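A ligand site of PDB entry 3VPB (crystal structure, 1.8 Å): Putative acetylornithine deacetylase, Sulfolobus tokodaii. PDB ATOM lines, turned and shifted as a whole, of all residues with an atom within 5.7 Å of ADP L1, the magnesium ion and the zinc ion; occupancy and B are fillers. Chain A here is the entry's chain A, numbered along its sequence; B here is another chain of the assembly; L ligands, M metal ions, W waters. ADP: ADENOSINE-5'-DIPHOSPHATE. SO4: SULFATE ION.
Water W2 lies within hydrogen-bond range of O3' of ADP L1 (2.8 Å), NH2 of Arg 192 (2.9 Å) and ND2 of Asn 202 (2.9 Å). Water W3 lies within hydrogen-bond range of the backbone carbonyl oxygen of Gly 131 (2.7 Å) and the chain-end carboxylate of Glu 56 of chain B (3.3 Å). Water W5 lies within hydrogen-bond range of O of Arg 135 (2.7 Å), O3B of ADP L1 (2.8 Å) and N of Ser 132 (3.5 Å). Water W4 lies within hydrogen-bond range of an oxygen (O2') of ADP L1 (2.8 Å), the side-chain amide nitrogen (NE2) of Gln 171 (3.0 Å) and the backbone carbonyl oxygen (O) of Trp 199 (3.2 Å). Water W1 lies within hydrogen-bond range of the side-chain carboxylate (OD1) of Asp 176, the side-chain amide nitrogen (ND2) of Asn 249 and an oxygen (O3') of ADP L1.
The magnesium ion is bound by O2A of ADP L1, OD1 of Asp 237, OE2 of Glu 250, O4 of SO4 L2, water W2 and O2B of ADP L1. The magnesium ion has six donor atoms within binding distance.
O of Ser 132 sits close to NH1 of Arg 135, 3.4 Å away. The side-chain carboxylate of Glu 250 lies close to the side-chain amino group of Lys 87, 3.4 Å away. The side-chain amino group of Lys 127 lies within hydrogen-bond range of the side-chain amide oxygen of Asn 249. The side-chain amino group of Lys 127 lies within hydrogen-bond range of the side-chain hydroxyl of Tyr 91 (3.4 Å). OH of Tyr 91 is in hydrogen-bond range of NE2 of Gln 167 (3.0 Å). The guanidinium group of Arg 192 lies within salt-bridge range of the side-chain carboxylate of Asp 176 (2.7 Å). The backbone NH of Gly 134 sits close to the side-chain amide nitrogen of Asn 202 (3.5 Å). The side-chain hydroxyl (OH) of Tyr 91 sits at hydrogen-bond distance from the backbone carbonyl oxygen (O) of Asn 249.
O1B of ADP L1 is bound to the zinc ion (1.9 Å). The zinc ion is bound by an oxygen (O2) of SO4 L2 (2.0 Å). The zinc ion is bound by water W3, 2.1 Å away. The side-chain carboxylate (OE2) of Glu 250 is bound to the zinc ion, 2.2 Å away. The side-chain carboxylate (OE1) of Glu 250 binds the zinc ion. The zinc ion is bound by OD1 of Asn 252 (2.3 Å). The zinc ion has six donor atoms within binding distance.
O of Gly 131 lies close to O1B of ADP L1, 3.4 Å away. Residues that only touch ADP L1: Ser 132 (3.4 Å), Tyr 169 (3.5 Å), Trp 133 (3.6 Å), Arg 200 (3.6 Å), Leu 239 (3.6 Å), Val 137 (3.6 Å), Ile 125 (3.7 Å), Arg 192 (3.8 Å) and Trp 199 (3.8 Å). Along chain A the residues within 4 Å of ADP L1 span positions 87 to 250.
N of Ile 170 sits at hydrogen-bond distance from N1 of ADP L1. O3' of ADP L1 sits at hydrogen-bond distance from OD1 of Asp 176 (2.6 Å). N6 of ADP L1 sits at hydrogen-bond distance from O of Glu 168, 2.9 Å away. The backbone NH of Ala 201 sits at hydrogen-bond distance from an oxygen (O2') of ADP L1, at 3.1 Å. The side-chain amide nitrogen (ND2) of Asn 249 is in hydrogen-bond range of an oxygen (O1A) of ADP L1 (3.1 Å). O3A of ADP L1 is in hydrogen-bond range of NZ of Lys 87 (3.3 Å). NZ of Lys 127 lies within salt-bridge range of O1A of ADP L1 (2.8 Å). O3B of ADP L1 is in hydrogen-bond range of N of Gly 134. A nitrogen (N6) of ADP L1 is in hydrogen-bond range of the side-chain amide oxygen (OE1) of Gln 167, at 2.9 Å. An oxygen (O2B) of ADP L1 sits close to the side-chain amide nitrogen (ND2) of Asn 202 (2.9 Å).
Residues that only touch the magnesium ion: Asn 202 (3.9 Å) and Arg 192 (3.999 Å).
Lys 87 touches the zinc ion (NZ to ZN, 3.97 Å). Gly 131 touches the zinc ion (O to ZN, 3.99 Å). Four residues have an atom within 4 Å of the zinc ion: Lys 87, Gly 131, Glu 250 and Asn 252.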
ATOM      1  N   LYS A  87       9.810   8.451   6.653  1.00  0.00           N
ATOM      2  CA  LYS A  87       8.872   7.329   6.547  1.00  0.00           C
ATOM      3  C   LYS A  87       9.544   5.958   6.734  1.00  0.00           C
ATOM      4  O   LYS A  87       8.908   5.036   7.223  1.00  0.00           O
ATOM      5  CB  LYS A  87       8.130   7.384   5.215  1.00  0.00           C
ATOM      6  CG  LYS A  87       7.152   8.544   5.096  1.00  0.00           C
ATOM      7  CD  LYS A  87       6.385   8.423   3.778  1.00  0.00           C
ATOM      8  CE  LYS A  87       5.253   9.457   3.744  1.00  0.00           C
ATOM      9  NZ  LYS A  87       5.762  10.826   3.533  1.00  0.00           N
ATOM     10  N   TYR A  91       8.358   3.442   9.538  1.00  0.00           N
ATOM     11  CA  TYR A  91       7.975   2.056   9.203  1.00  0.00           C
ATOM     12  C   TYR A  91       8.779   1.057   9.972  1.00  0.00           C
ATOM     13  O   TYR A  91       8.234   0.041  10.409  1.00  0.00           O
ATOM     14  CB  TYR A  91       8.136   1.770   7.703  1.00  0.00           C
ATOM     15  CG  TYR A  91       7.096   2.422   6.838  1.00  0.00           C
ATOM     16  CD1 TYR A  91       7.447   2.929   5.579  1.00  0.00           C
ATOM     17  CD2 TYR A  91       5.769   2.539   7.261  1.00  0.00           C
ATOM     18  CE1 TYR A  91       6.504   3.521   4.778  1.00  0.00           C
ATOM     19  CE2 TYR A  91       4.799   3.117   6.460  1.00  0.00           C
ATOM     20  CZ  TYR A  91       5.180   3.617   5.214  1.00  0.00           C
ATOM     21  OH  TYR A  91       4.248   4.185   4.403  1.00  0.00           O
ATOM     22  N   PRO A 102       1.873  -0.685   5.000  1.00  0.00           N
ATOM     23  CA  PRO A 102       1.781  -1.303   3.686  1.00  0.00           C
ATOM     24  C   PRO A 102       2.960  -2.220   3.415  1.00  0.00           C
ATOM     25  O   PRO A 102       4.080  -1.952   3.885  1.00  0.00           O
ATOM     26  CB  PRO A 102       1.850  -0.087   2.715  1.00  0.00           C
ATOM     27  CG  PRO A 102       1.415   1.092   3.532  1.00  0.00           C
ATOM     28  CD  PRO A 102       1.901   0.787   4.943  1.00  0.00           C
ATOM     29  N   ILE A 125       3.014   1.770  -5.396  1.00  0.00           N
ATOM     30  CA  ILE A 125       3.344   3.153  -5.015  1.00  0.00           C
ATOM     31  C   ILE A 125       4.846   3.264  -4.772  1.00  0.00           C
ATOM     32  O   ILE A 125       5.423   2.410  -4.147  1.00  0.00           O
ATOM     33  CB  ILE A 125       2.519   3.577  -3.762  1.00  0.00           C
ATOM     34  CG1 ILE A 125       1.055   3.853  -4.176  1.00  0.00           C
ATOM     35  CG2 ILE A 125       3.175   4.750  -3.007  1.00  0.00           C
ATOM     36  CD1 ILE A 125       0.815   5.270  -4.855  1.00  0.00           C
ATOM     37  N   LYS A 127       7.399   6.108  -3.211  1.00  0.00           N
ATOM     38  CA  LYS A 127       7.565   7.443  -2.633  1.00  0.00           C
ATOM     39  C   LYS A 127       8.894   7.564  -1.887  1.00  0.00           C
ATOM     40  O   LYS A 127       9.435   6.574  -1.410  1.00  0.00           O
ATOM     41  CB  LYS A 127       6.372   7.805  -1.731  1.00  0.00           C
ATOM     42  CG  LYS A 127       6.179   6.885  -0.518  1.00  0.00           C
ATOM     43  CD  LYS A 127       4.763   7.009   0.051  1.00  0.00           C
ATOM     44  CE  LYS A 127       4.588   6.102   1.295  1.00  0.00           C
ATOM     45  NZ  LYS A 127       3.133   5.923   1.694  1.00  0.00           N
ATOM     46  N   GLY A 131       9.216  14.137   2.707  1.00  0.00           N
ATOM     47  CA  GLY A 131       8.278  14.856   1.888  1.00  0.00           C
ATOM     48  C   GLY A 131       6.955  14.902   2.602  1.00  0.00           C
ATOM     49  O   GLY A 131       6.708  14.140   3.557  1.00  0.00           O
ATOM     50  N   SER A 132       6.113  15.808   2.151  1.00  0.00           N
ATOM     51  CA  SER A 132       4.777  16.001   2.686  1.00  0.00           C
ATOM     52  C   SER A 132       3.896  16.454   1.529  1.00  0.00           C
ATOM     53  O   SER A 132       4.396  16.669   0.413  1.00  0.00           O
ATOM     54  CB  SER A 132       4.810  17.062   3.797  1.00  0.00           C
ATOM     55  OG  SER A 132       3.568  17.182   4.467  1.00  0.00           O
ATOM     56  N   TRP A 133       2.594  16.593   1.777  1.00  0.00           N
ATOM     57  CA  TRP A 133       1.634  17.131   0.793  1.00  0.00           C
ATOM     58  C   TRP A 133       1.532  16.350  -0.521  1.00  0.00           C
ATOM     59  O   TRP A 133       1.078  16.867  -1.539  1.00  0.00           O
ATOM     60  CB  TRP A 133       1.935  18.609   0.468  1.00  0.00           C
ATOM     61  CG  TRP A 133       1.924  19.554   1.628  1.00  0.00           C
ATOM     62  CD1 TRP A 133       1.105  19.512   2.733  1.00  0.00           C
ATOM     63  CD2 TRP A 133       2.722  20.727   1.770  1.00  0.00           C
ATOM     64  NE1 TRP A 133       1.376  20.573   3.567  1.00  0.00           N
ATOM     65  CE2 TRP A 133       2.340  21.351   2.983  1.00  0.00           C
ATOM     66  CE3 TRP A 133       3.702  21.347   0.970  1.00  0.00           C
ATOM     67  CZ2 TRP A 133       2.947  22.530   3.444  1.00  0.00           C
ATOM     68  CZ3 TRP A 133       4.295  22.518   1.436  1.00  0.00           C
ATOM     69  CH2 TRP A 133       3.906  23.097   2.649  1.00  0.00           C
ATOM     70  N   GLY A 134       1.951  15.086  -0.478  1.00  0.00           N
ATOM     71  CA  GLY A 134       1.844  14.198  -1.630  1.00  0.00           C
ATOM     72  C   GLY A 134       3.012  14.325  -2.598  1.00  0.00           C
ATOM     73  O   GLY A 134       3.034  13.642  -3.602  1.00  0.00           O
ATOM     74  N   ARG A 135       3.982  15.178  -2.256  1.00  0.00           N
ATOM     75  CA  ARG A 135       5.109  15.495  -3.142  1.00  0.00           C
ATOM     76  C   ARG A 135       5.937  14.235  -3.447  1.00  0.00           C
ATOM     77  O   ARG A 135       6.430  13.552  -2.534  1.00  0.00           O
ATOM     78  CB  ARG A 135       5.972  16.600  -2.510  1.00  0.00           C
ATOM     79  CG  ARG A 135       6.819  17.415  -3.484  1.00  0.00           C
ATOM     80  CD  ARG A 135       7.331  18.692  -2.792  1.00  0.00           C
ATOM     81  NE  ARG A 135       7.950  18.382  -1.496  1.00  0.00           N
ATOM     82  CZ  ARG A 135       7.458  18.727  -0.308  1.00  0.00           C
ATOM     83  NH1 ARG A 135       6.322  19.413  -0.226  1.00  0.00           N
ATOM     84  NH2 ARG A 135       8.091  18.385   0.808  1.00  0.00           N
ATOM     85  N   VAL A 137       4.975  11.344  -4.446  1.00  0.00           N
ATOM     86  CA  VAL A 137       4.296  10.061  -4.220  1.00  0.00           C
ATOM     87  C   VAL A 137       3.755   9.672  -5.595  1.00  0.00           C
ATOM     88  O   VAL A 137       2.854  10.351  -6.116  1.00  0.00           O
ATOM     89  CB  VAL A 137       3.146  10.168  -3.208  1.00  0.00           C
ATOM     90  CG1 VAL A 137       2.441   8.798  -3.049  1.00  0.00           C
ATOM     91  CG2 VAL A 137       3.663  10.658  -1.801  1.00  0.00           C
ATOM     92  N   GLN A 167       5.799   0.167  -2.529  1.00  0.00           N
ATOM     93  CA  GLN A 167       4.740  -0.360  -1.642  1.00  0.00           C
ATOM     94  C   GLN A 167       3.555  -0.850  -2.437  1.00  0.00           C
ATOM     95  O   GLN A 167       3.280  -0.361  -3.564  1.00  0.00           O
ATOM     96  CB  GLN A 167       4.129   0.721  -0.753  1.00  0.00           C
ATOM     97  CG  GLN A 167       4.999   1.618  -0.027  1.00  0.00           C
ATOM     98  CD  GLN A 167       4.241   2.368   1.009  1.00  0.00           C
ATOM     99  OE1 GLN A 167       3.284   3.129   0.719  1.00  0.00           O
ATOM    100  NE2 GLN A 167       4.663   2.188   2.257  1.00  0.00           N
ATOM    101  N   GLU A 168       2.830  -1.760  -1.833  1.00  0.00           N
ATOM    102  CA  GLU A 168       1.514  -2.139  -2.374  1.00  0.00           C
ATOM    103  C   GLU A 168       0.628  -0.889  -2.415  1.00  0.00           C
ATOM    104  O   GLU A 168       0.723  -0.004  -1.567  1.00  0.00           O
ATOM    105  CB  GLU A 168       0.846  -3.227  -1.522  1.00  0.00           C
ATOM    106  CG  GLU A 168       0.692  -2.891  -0.053  1.00  0.00           C
ATOM    107  CD  GLU A 168      -0.143  -3.905   0.697  1.00  0.00           C
ATOM    108  OE1 GLU A 168      -1.142  -4.404   0.115  1.00  0.00           O
ATOM    109  OE2 GLU A 168       0.165  -4.148   1.877  1.00  0.00           O
ATOM    110  N   TYR A 169      -0.248  -0.845  -3.416  1.00  0.00           N
ATOM    111  CA  TYR A 169      -1.193   0.235  -3.546  1.00  0.00           C
ATOM    112  C   TYR A 169      -2.457  -0.145  -2.799  1.00  0.00           C
ATOM    113  O   TYR A 169      -3.065  -1.145  -3.143  1.00  0.00           O
ATOM    114  CB  TYR A 169      -1.454   0.460  -5.027  1.00  0.00           C
ATOM    115  CG  TYR A 169      -2.491   1.508  -5.296  1.00  0.00           C
ATOM    116  CD1 TYR A 169      -2.256   2.846  -4.962  1.00  0.00           C
ATOM    117  CD2 TYR A 169      -3.706   1.171  -5.858  1.00  0.00           C
ATOM    118  CE1 TYR A 169      -3.213   3.824  -5.207  1.00  0.00           C
ATOM    119  CE2 TYR A 169      -4.671   2.128  -6.103  1.00  0.00           C
ATOM    120  CZ  TYR A 169      -4.401   3.447  -5.805  1.00  0.00           C
ATOM    121  OH  TYR A 169      -5.366   4.380  -6.073  1.00  0.00           O
ATOM    122  N   ILE A 170      -2.839   0.631  -1.783  1.00  0.00           N
ATOM    123  CA  ILE A 170      -3.988   0.322  -0.964  1.00  0.00           C
ATOM    124  C   ILE A 170      -5.014   1.414  -1.100  1.00  0.00           C
ATOM    125  O   ILE A 170      -4.902   2.497  -0.480  1.00  0.00           O
ATOM    126  CB  ILE A 170      -3.616   0.130   0.550  1.00  0.00           C
ATOM    127  CG1 ILE A 170      -2.455  -0.866   0.695  1.00  0.00           C
ATOM    128  CG2 ILE A 170      -4.851  -0.339   1.282  1.00  0.00           C
ATOM    129  CD1 ILE A 170      -1.924  -0.977   2.158  1.00  0.00           C
ATOM    130  N   GLN A 171      -6.022   1.161  -1.936  1.00  0.00           N
ATOM    131  CA  GLN A 171      -7.095   2.133  -2.057  1.00  0.00           C
ATOM    132  C   GLN A 171      -8.273   1.520  -2.785  1.00  0.00           C
ATOM    133  O   GLN A 171      -8.177   1.181  -3.997  1.00  0.00           O
ATOM    134  CB  GLN A 171      -6.638   3.391  -2.839  1.00  0.00           C
ATOM    135  CG  GLN A 171      -7.701   4.498  -2.951  1.00  0.00           C
ATOM    136  CD  GLN A 171      -8.131   4.989  -1.608  1.00  0.00           C
ATOM    137  OE1 GLN A 171      -9.284   4.840  -1.227  1.00  0.00           O
ATOM    138  NE2 GLN A 171      -7.215   5.594  -0.889  1.00  0.00           N
ATOM    139  N   ASP A 176      -8.480   8.615   2.396  1.00  0.00           N
ATOM    140  CA  ASP A 176      -7.728   8.058   3.485  1.00  0.00           C
ATOM    141  C   ASP A 176      -8.217   8.620   4.830  1.00  0.00           C
ATOM    142  O   ASP A 176      -9.140   9.439   4.883  1.00  0.00           O
ATOM    143  CB  ASP A 176      -6.202   8.134   3.226  1.00  0.00           C
ATOM    144  CG  ASP A 176      -5.605   9.469   3.513  1.00  0.00           C
ATOM    145  OD1 ASP A 176      -4.344   9.565   3.446  1.00  0.00           O
ATOM    146  OD2 ASP A 176      -6.362  10.418   3.807  1.00  0.00           O
ATOM    147  N   ARG A 178      -7.308  10.474   8.410  1.00  0.00           N
ATOM    148  CA  ARG A 178      -6.387  11.308   9.147  1.00  0.00           C
ATOM    149  C   ARG A 178      -6.858  11.441  10.586  1.00  0.00           C
ATOM    150  O   ARG A 178      -7.983  11.866  10.859  1.00  0.00           O
ATOM    151  CB  ARG A 178      -6.269  12.680   8.457  1.00  0.00           C
ATOM    152  CG  ARG A 178      -5.734  13.839   9.287  1.00  0.00           C
ATOM    153  CD  ARG A 178      -4.365  13.578   9.905  1.00  0.00           C
ATOM    154  NE  ARG A 178      -3.244  13.417   8.974  1.00  0.00           N
ATOM    155  CZ  ARG A 178      -2.501  14.418   8.505  1.00  0.00           C
ATOM    156  NH1 ARG A 178      -2.741  15.697   8.819  1.00  0.00           N
ATOM    157  NH2 ARG A 178      -1.486  14.141   7.716  1.00  0.00           N
ATOM    158  N   ARG A 192     -10.173  12.073   4.450  1.00  0.00           N
ATOM    159  CA  ARG A 192      -9.793  12.968   3.343  1.00  0.00           C
ATOM    160  C   ARG A 192     -10.189  12.316   2.035  1.00  0.00           C
ATOM    161  O   ARG A 192      -9.615  11.290   1.666  1.00  0.00           O
ATOM    162  CB  ARG A 192      -8.294  13.226   3.377  1.00  0.00           C
ATOM    163  CG  ARG A 192      -7.864  13.946   4.621  1.00  0.00           C
ATOM    164  CD  ARG A 192      -6.351  14.241   4.618  1.00  0.00           C
ATOM    165  NE  ARG A 192      -5.593  12.993   4.641  1.00  0.00           N
ATOM    166  CZ  ARG A 192      -4.293  12.918   4.868  1.00  0.00           C
ATOM    167  NH1 ARG A 192      -3.572  14.026   5.080  1.00  0.00           N
ATOM    168  NH2 ARG A 192      -3.708  11.724   4.901  1.00  0.00           N
ATOM    169  N   ILE A 194     -10.500  11.795  -1.916  1.00  0.00           N
ATOM    170  CA  ILE A 194      -9.695  12.057  -3.109  1.00  0.00           C
ATOM    171  C   ILE A 194     -10.506  12.815  -4.169  1.00  0.00           C
ATOM    172  O   ILE A 194     -11.614  12.380  -4.559  1.00  0.00           O
ATOM    173  CB  ILE A 194      -9.102  10.737  -3.667  1.00  0.00           C
ATOM    174  CG1 ILE A 194      -8.205  10.114  -2.586  1.00  0.00           C
ATOM    175  CG2 ILE A 194      -8.329  10.977  -4.953  1.00  0.00           C
ATOM    176  CD1 ILE A 194      -7.798   8.650  -2.839  1.00  0.00           C
ATOM    177  N   TRP A 199      -4.813  10.851  -7.311  1.00  0.00           N
ATOM    178  CA  TRP A 199      -4.625   9.550  -6.675  1.00  0.00           C
ATOM    179  C   TRP A 199      -4.252   9.722  -5.192  1.00  0.00           C
ATOM    180  O   TRP A 199      -4.094   8.746  -4.442  1.00  0.00           O
ATOM    181  CB  TRP A 199      -3.560   8.711  -7.417  1.00  0.00           C
ATOM    182  CG  TRP A 199      -2.177   9.274  -7.371  1.00  0.00           C
ATOM    183  CD1 TRP A 199      -1.147   8.821  -6.603  1.00  0.00           C
ATOM    184  CD2 TRP A 199      -1.649  10.380  -8.124  1.00  0.00           C
ATOM    185  NE1 TRP A 199      -0.018   9.582  -6.826  1.00  0.00           N
ATOM    186  CE2 TRP A 199      -0.301  10.552  -7.742  1.00  0.00           C
ATOM    187  CE3 TRP A 199      -2.200  11.272  -9.072  1.00  0.00           C
ATOM    188  CZ2 TRP A 199       0.518  11.560  -8.286  1.00  0.00           C
ATOM    189  CZ3 TRP A 199      -1.394  12.276  -9.597  1.00  0.00           C
ATOM    190  CH2 TRP A 199      -0.043  12.399  -9.215  1.00  0.00           C
ATOM    191  N   ARG A 200      -4.088  10.983  -4.793  1.00  0.00           N
ATOM    192  CA  ARG A 200      -3.620  11.324  -3.451  1.00  0.00           C
ATOM    193  C   ARG A 200      -4.710  12.072  -2.699  1.00  0.00           C
ATOM    194  O   ARG A 200      -5.455  12.852  -3.283  1.00  0.00           O
ATOM    195  CB  ARG A 200      -2.355  12.172  -3.535  1.00  0.00           C
ATOM    196  CG  ARG A 200      -1.220  11.426  -4.235  1.00  0.00           C
ATOM    197  CD  ARG A 200      -0.123  12.361  -4.604  1.00  0.00           C
ATOM    198  NE  ARG A 200      -0.587  13.291  -5.644  1.00  0.00           N
ATOM    199  CZ  ARG A 200       0.160  14.251  -6.154  1.00  0.00           C
ATOM    200  NH1 ARG A 200       1.433  14.395  -5.751  1.00  0.00           N
ATOM    201  NH2 ARG A 200      -0.341  15.052  -7.081  1.00  0.00           N
ATOM    202  N   ALA A 201      -4.803  11.810  -1.399  1.00  0.00           N
ATOM    203  CA  ALA A 201      -5.909  12.324  -0.625  1.00  0.00           C
ATOM    204  C   ALA A 201      -5.630  13.663   0.039  1.00  0.00           C
ATOM    205  O   ALA A 201      -6.547  14.297   0.553  1.00  0.00           O
ATOM    206  CB  ALA A 201      -6.312  11.288   0.447  1.00  0.00           C
ATOM    207  N   ASN A 202      -4.370  14.111   0.013  1.00  0.00           N
ATOM    208  CA  ASN A 202      -3.982  15.312   0.763  1.00  0.00           C
ATOM    209  C   ASN A 202      -4.912  16.491   0.571  1.00  0.00           C
ATOM    210  O   ASN A 202      -5.277  16.861  -0.580  1.00  0.00           O
ATOM    211  CB  ASN A 202      -2.549  15.731   0.427  1.00  0.00           C
ATOM    212  CG  ASN A 202      -1.551  14.592   0.582  1.00  0.00           C
ATOM    213  OD1 ASN A 202      -1.504  13.685  -0.244  1.00  0.00           O
ATOM    214  ND2 ASN A 202      -0.741  14.651   1.643  1.00  0.00           N
ATOM    215  N   ASP A 237      -1.749   8.978   9.372  1.00  0.00           N
ATOM    216  CA  ASP A 237      -2.419   8.717   8.104  1.00  0.00           C
ATOM    217  C   ASP A 237      -2.670   7.206   8.043  1.00  0.00           C
ATOM    218  O   ASP A 237      -1.746   6.427   8.187  1.00  0.00           O
ATOM    219  CB  ASP A 237      -1.538   9.089   6.895  1.00  0.00           C
ATOM    220  CG  ASP A 237      -1.367  10.585   6.660  1.00  0.00           C
ATOM    221  OD1 ASP A 237      -1.074  10.966   5.478  1.00  0.00           O
ATOM    222  OD2 ASP A 237      -1.483  11.390   7.595  1.00  0.00           O
ATOM    223  N   LEU A 239      -4.612   3.971   5.858  1.00  0.00           N
ATOM    224  CA  LEU A 239      -5.232   3.451   4.633  1.00  0.00           C
ATOM    225  C   LEU A 239      -6.123   2.272   5.009  1.00  0.00           C
ATOM    226  O   LEU A 239      -5.923   1.628   6.053  1.00  0.00           O
ATOM    227  CB  LEU A 239      -4.175   3.025   3.614  1.00  0.00           C
ATOM    228  CG  LEU A 239      -3.279   4.172   3.113  1.00  0.00           C
ATOM    229  CD1 LEU A 239      -1.993   3.613   2.490  1.00  0.00           C
ATOM    230  CD2 LEU A 239      -4.045   5.042   2.123  1.00  0.00           C
ATOM    231  N   ASN A 249      -0.051   4.318   7.427  1.00  0.00           N
ATOM    232  CA  ASN A 249       0.768   4.801   6.305  1.00  0.00           C
ATOM    233  C   ASN A 249       1.889   5.760   6.718  1.00  0.00           C
ATOM    234  O   ASN A 249       3.019   5.638   6.253  1.00  0.00           O
ATOM    235  CB  ASN A 249      -0.136   5.457   5.284  1.00  0.00           C
ATOM    236  CG  ASN A 249       0.569   5.718   3.986  1.00  0.00           C
ATOM    237  OD1 ASN A 249       1.519   5.016   3.646  1.00  0.00           O
ATOM    238  ND2 ASN A 249       0.085   6.712   3.229  1.00  0.00           N
ATOM    239  N   GLU A 250       1.601   6.708   7.584  1.00  0.00           N
ATOM    240  CA  GLU A 250       2.641   7.646   8.075  1.00  0.00           C
ATOM    241  C   GLU A 250       2.141   8.379   9.309  1.00  0.00           C
ATOM    242  O   GLU A 250       0.954   8.339   9.647  1.00  0.00           O
ATOM    243  CB  GLU A 250       3.066   8.654   6.994  1.00  0.00           C
ATOM    244  CG  GLU A 250       2.004   9.672   6.685  1.00  0.00           C
ATOM    245  CD  GLU A 250       2.549  10.970   6.124  1.00  0.00           C
ATOM    246  OE1 GLU A 250       3.766  11.235   6.295  1.00  0.00           O
ATOM    247  OE2 GLU A 250       1.739  11.748   5.551  1.00  0.00           O
ATOM    248  N   LEU A 251       3.076   9.034   9.988  1.00  0.00           N
ATOM    249  CA  LEU A 251       2.816   9.950  11.098  1.00  0.00           C
ATOM    250  C   LEU A 251       3.502  11.238  10.698  1.00  0.00           C
ATOM    251  O   LEU A 251       4.495  11.201   9.972  1.00  0.00           O
ATOM    252  CB  LEU A 251       3.486   9.442  12.387  1.00  0.00           C
ATOM    253  CG  LEU A 251       3.096   8.265  13.283  1.00  0.00           C
ATOM    254  CD1 LEU A 251       2.206   8.689  14.494  1.00  0.00           C
ATOM    255  CD2 LEU A 251       2.588   7.029  12.577  1.00  0.00           C
ATOM    256  N   ASN A 252       2.974  12.377  11.137  1.00  0.00           N
ATOM    257  CA  ASN A 252       3.599  13.666  10.850  1.00  0.00           C
ATOM    258  C   ASN A 252       3.859  14.442  12.119  1.00  0.00           C
ATOM    259  O   ASN A 252       3.015  14.462  13.036  1.00  0.00           O
ATOM    260  CB  ASN A 252       2.740  14.483   9.922  1.00  0.00           C
ATOM    261  CG  ASN A 252       2.445  13.758   8.628  1.00  0.00           C
ATOM    262  OD1 ASN A 252       3.196  13.890   7.655  1.00  0.00           O
ATOM    263  ND2 ASN A 252       1.368  12.959   8.607  1.00  0.00           N
ATOM    264  N   GLU B  56       4.131  18.816   6.702  1.00  0.00           N
ATOM    265  CA  GLU B  56       3.882  18.289   8.034  1.00  0.00           C
ATOM    266  C   GLU B  56       4.974  17.338   8.490  1.00  0.00           C
ATOM    267  O   GLU B  56       5.159  17.106   9.701  1.00  0.00           O
ATOM    268  CB  GLU B  56       2.590  17.489   8.025  1.00  0.00           C
ATOM    269  CG  GLU B  56       1.370  18.287   7.823  1.00  0.00           C
ATOM    270  CD  GLU B  56       0.203  17.613   8.481  1.00  0.00           C
ATOM    271  OE1 GLU B  56      -0.897  17.809   8.007  1.00  0.00           O
ATOM    272  OE2 GLU B  56       0.402  16.860   9.485  1.00  0.00           O
ATOM    273  OXT GLU B  56       5.653  16.755   7.631  1.00  0.00           O
HETATM  274  PB  ADP L   1       2.810  12.543   2.453  1.00  0.00           P
HETATM  275  O1B ADP L   1       3.697  12.650   3.637  1.00  0.00           O
HETATM  276  O2B ADP L   1       1.359  12.903   2.715  1.00  0.00           O
HETATM  277  O3B ADP L   1       3.313  13.163   1.181  1.00  0.00           O
HETATM  278  PA  ADP L   1       1.693   9.888   2.109  1.00  0.00           P
HETATM  279  O1A ADP L   1       2.388   8.555   2.228  1.00  0.00           O
HETATM  280  O2A ADP L   1       0.720  10.305   3.170  1.00  0.00           O
HETATM  281  O3A ADP L   1       2.866  10.993   2.019  1.00  0.00           O
HETATM  282  O5' ADP L   1       1.038   9.931   0.617  1.00  0.00           O
HETATM  283  C5' ADP L   1       0.116  10.956   0.210  1.00  0.00           C
HETATM  284  C4' ADP L   1      -1.190  10.353  -0.277  1.00  0.00           C
HETATM  285  O4' ADP L   1      -0.886   9.402  -1.286  1.00  0.00           O
HETATM  286  C3' ADP L   1      -1.939   9.534   0.765  1.00  0.00           C
HETATM  287  O3' ADP L   1      -2.854  10.348   1.485  1.00  0.00           O
HETATM  288  C2' ADP L   1      -2.635   8.458  -0.051  1.00  0.00           C
HETATM  289  O2' ADP L   1      -3.824   8.985  -0.652  1.00  0.00           O
HETATM  290  C1' ADP L   1      -1.667   8.225  -1.160  1.00  0.00           C
HETATM  291  N9  ADP L   1      -0.813   7.058  -0.818  1.00  0.00           N
HETATM  292  C8  ADP L   1       0.453   7.062  -0.281  1.00  0.00           C
HETATM  293  N7  ADP L   1       0.889   5.778  -0.145  1.00  0.00           N
HETATM  294  C5  ADP L   1      -0.090   4.966  -0.603  1.00  0.00           C
HETATM  295  C6  ADP L   1      -0.304   3.497  -0.705  1.00  0.00           C
HETATM  296  N6  ADP L   1       0.681   2.663  -0.344  1.00  0.00           N
HETATM  297  N1  ADP L   1      -1.466   3.044  -1.224  1.00  0.00           N
HETATM  298  C2  ADP L   1      -2.444   3.898  -1.607  1.00  0.00           C
HETATM  299  N3  ADP L   1      -2.342   5.243  -1.501  1.00  0.00           N
HETATM  300  C4  ADP L   1      -1.202   5.810  -1.022  1.00  0.00           C
HETATM  301  S   SO4 L   2       0.669  15.058   5.049  1.00  0.00           S
HETATM  302  O1  SO4 L   2       0.390  16.025   3.976  1.00  0.00           O
HETATM  303  O2  SO4 L   2       2.120  14.840   5.042  1.00  0.00           O
HETATM  304  O3  SO4 L   2       0.310  15.741   6.269  1.00  0.00           O
HETATM  305  O4  SO4 L   2      -0.121  13.829   4.848  1.00  0.00           O
HETATM  306 MG    MG M   1       0.221  11.881   4.172  1.00  0.00          MG
HETATM  307 ZN    ZN M   2       3.285  13.287   5.419  1.00  0.00          ZN
HETATM  308  O   HOH W   1      -1.998   8.399   3.746  1.00  0.00           O
HETATM  309  O   HOH W   2      -1.544  12.215   3.061  1.00  0.00           O
HETATM  310  O   HOH W   3       5.197  14.079   5.740  1.00  0.00           O
HETATM  311  O   HOH W   4      -4.740   6.743  -2.098  1.00  0.00           O
HETATM  312  O   HOH W   5       5.840  13.010   0.075  1.00  0.00           O
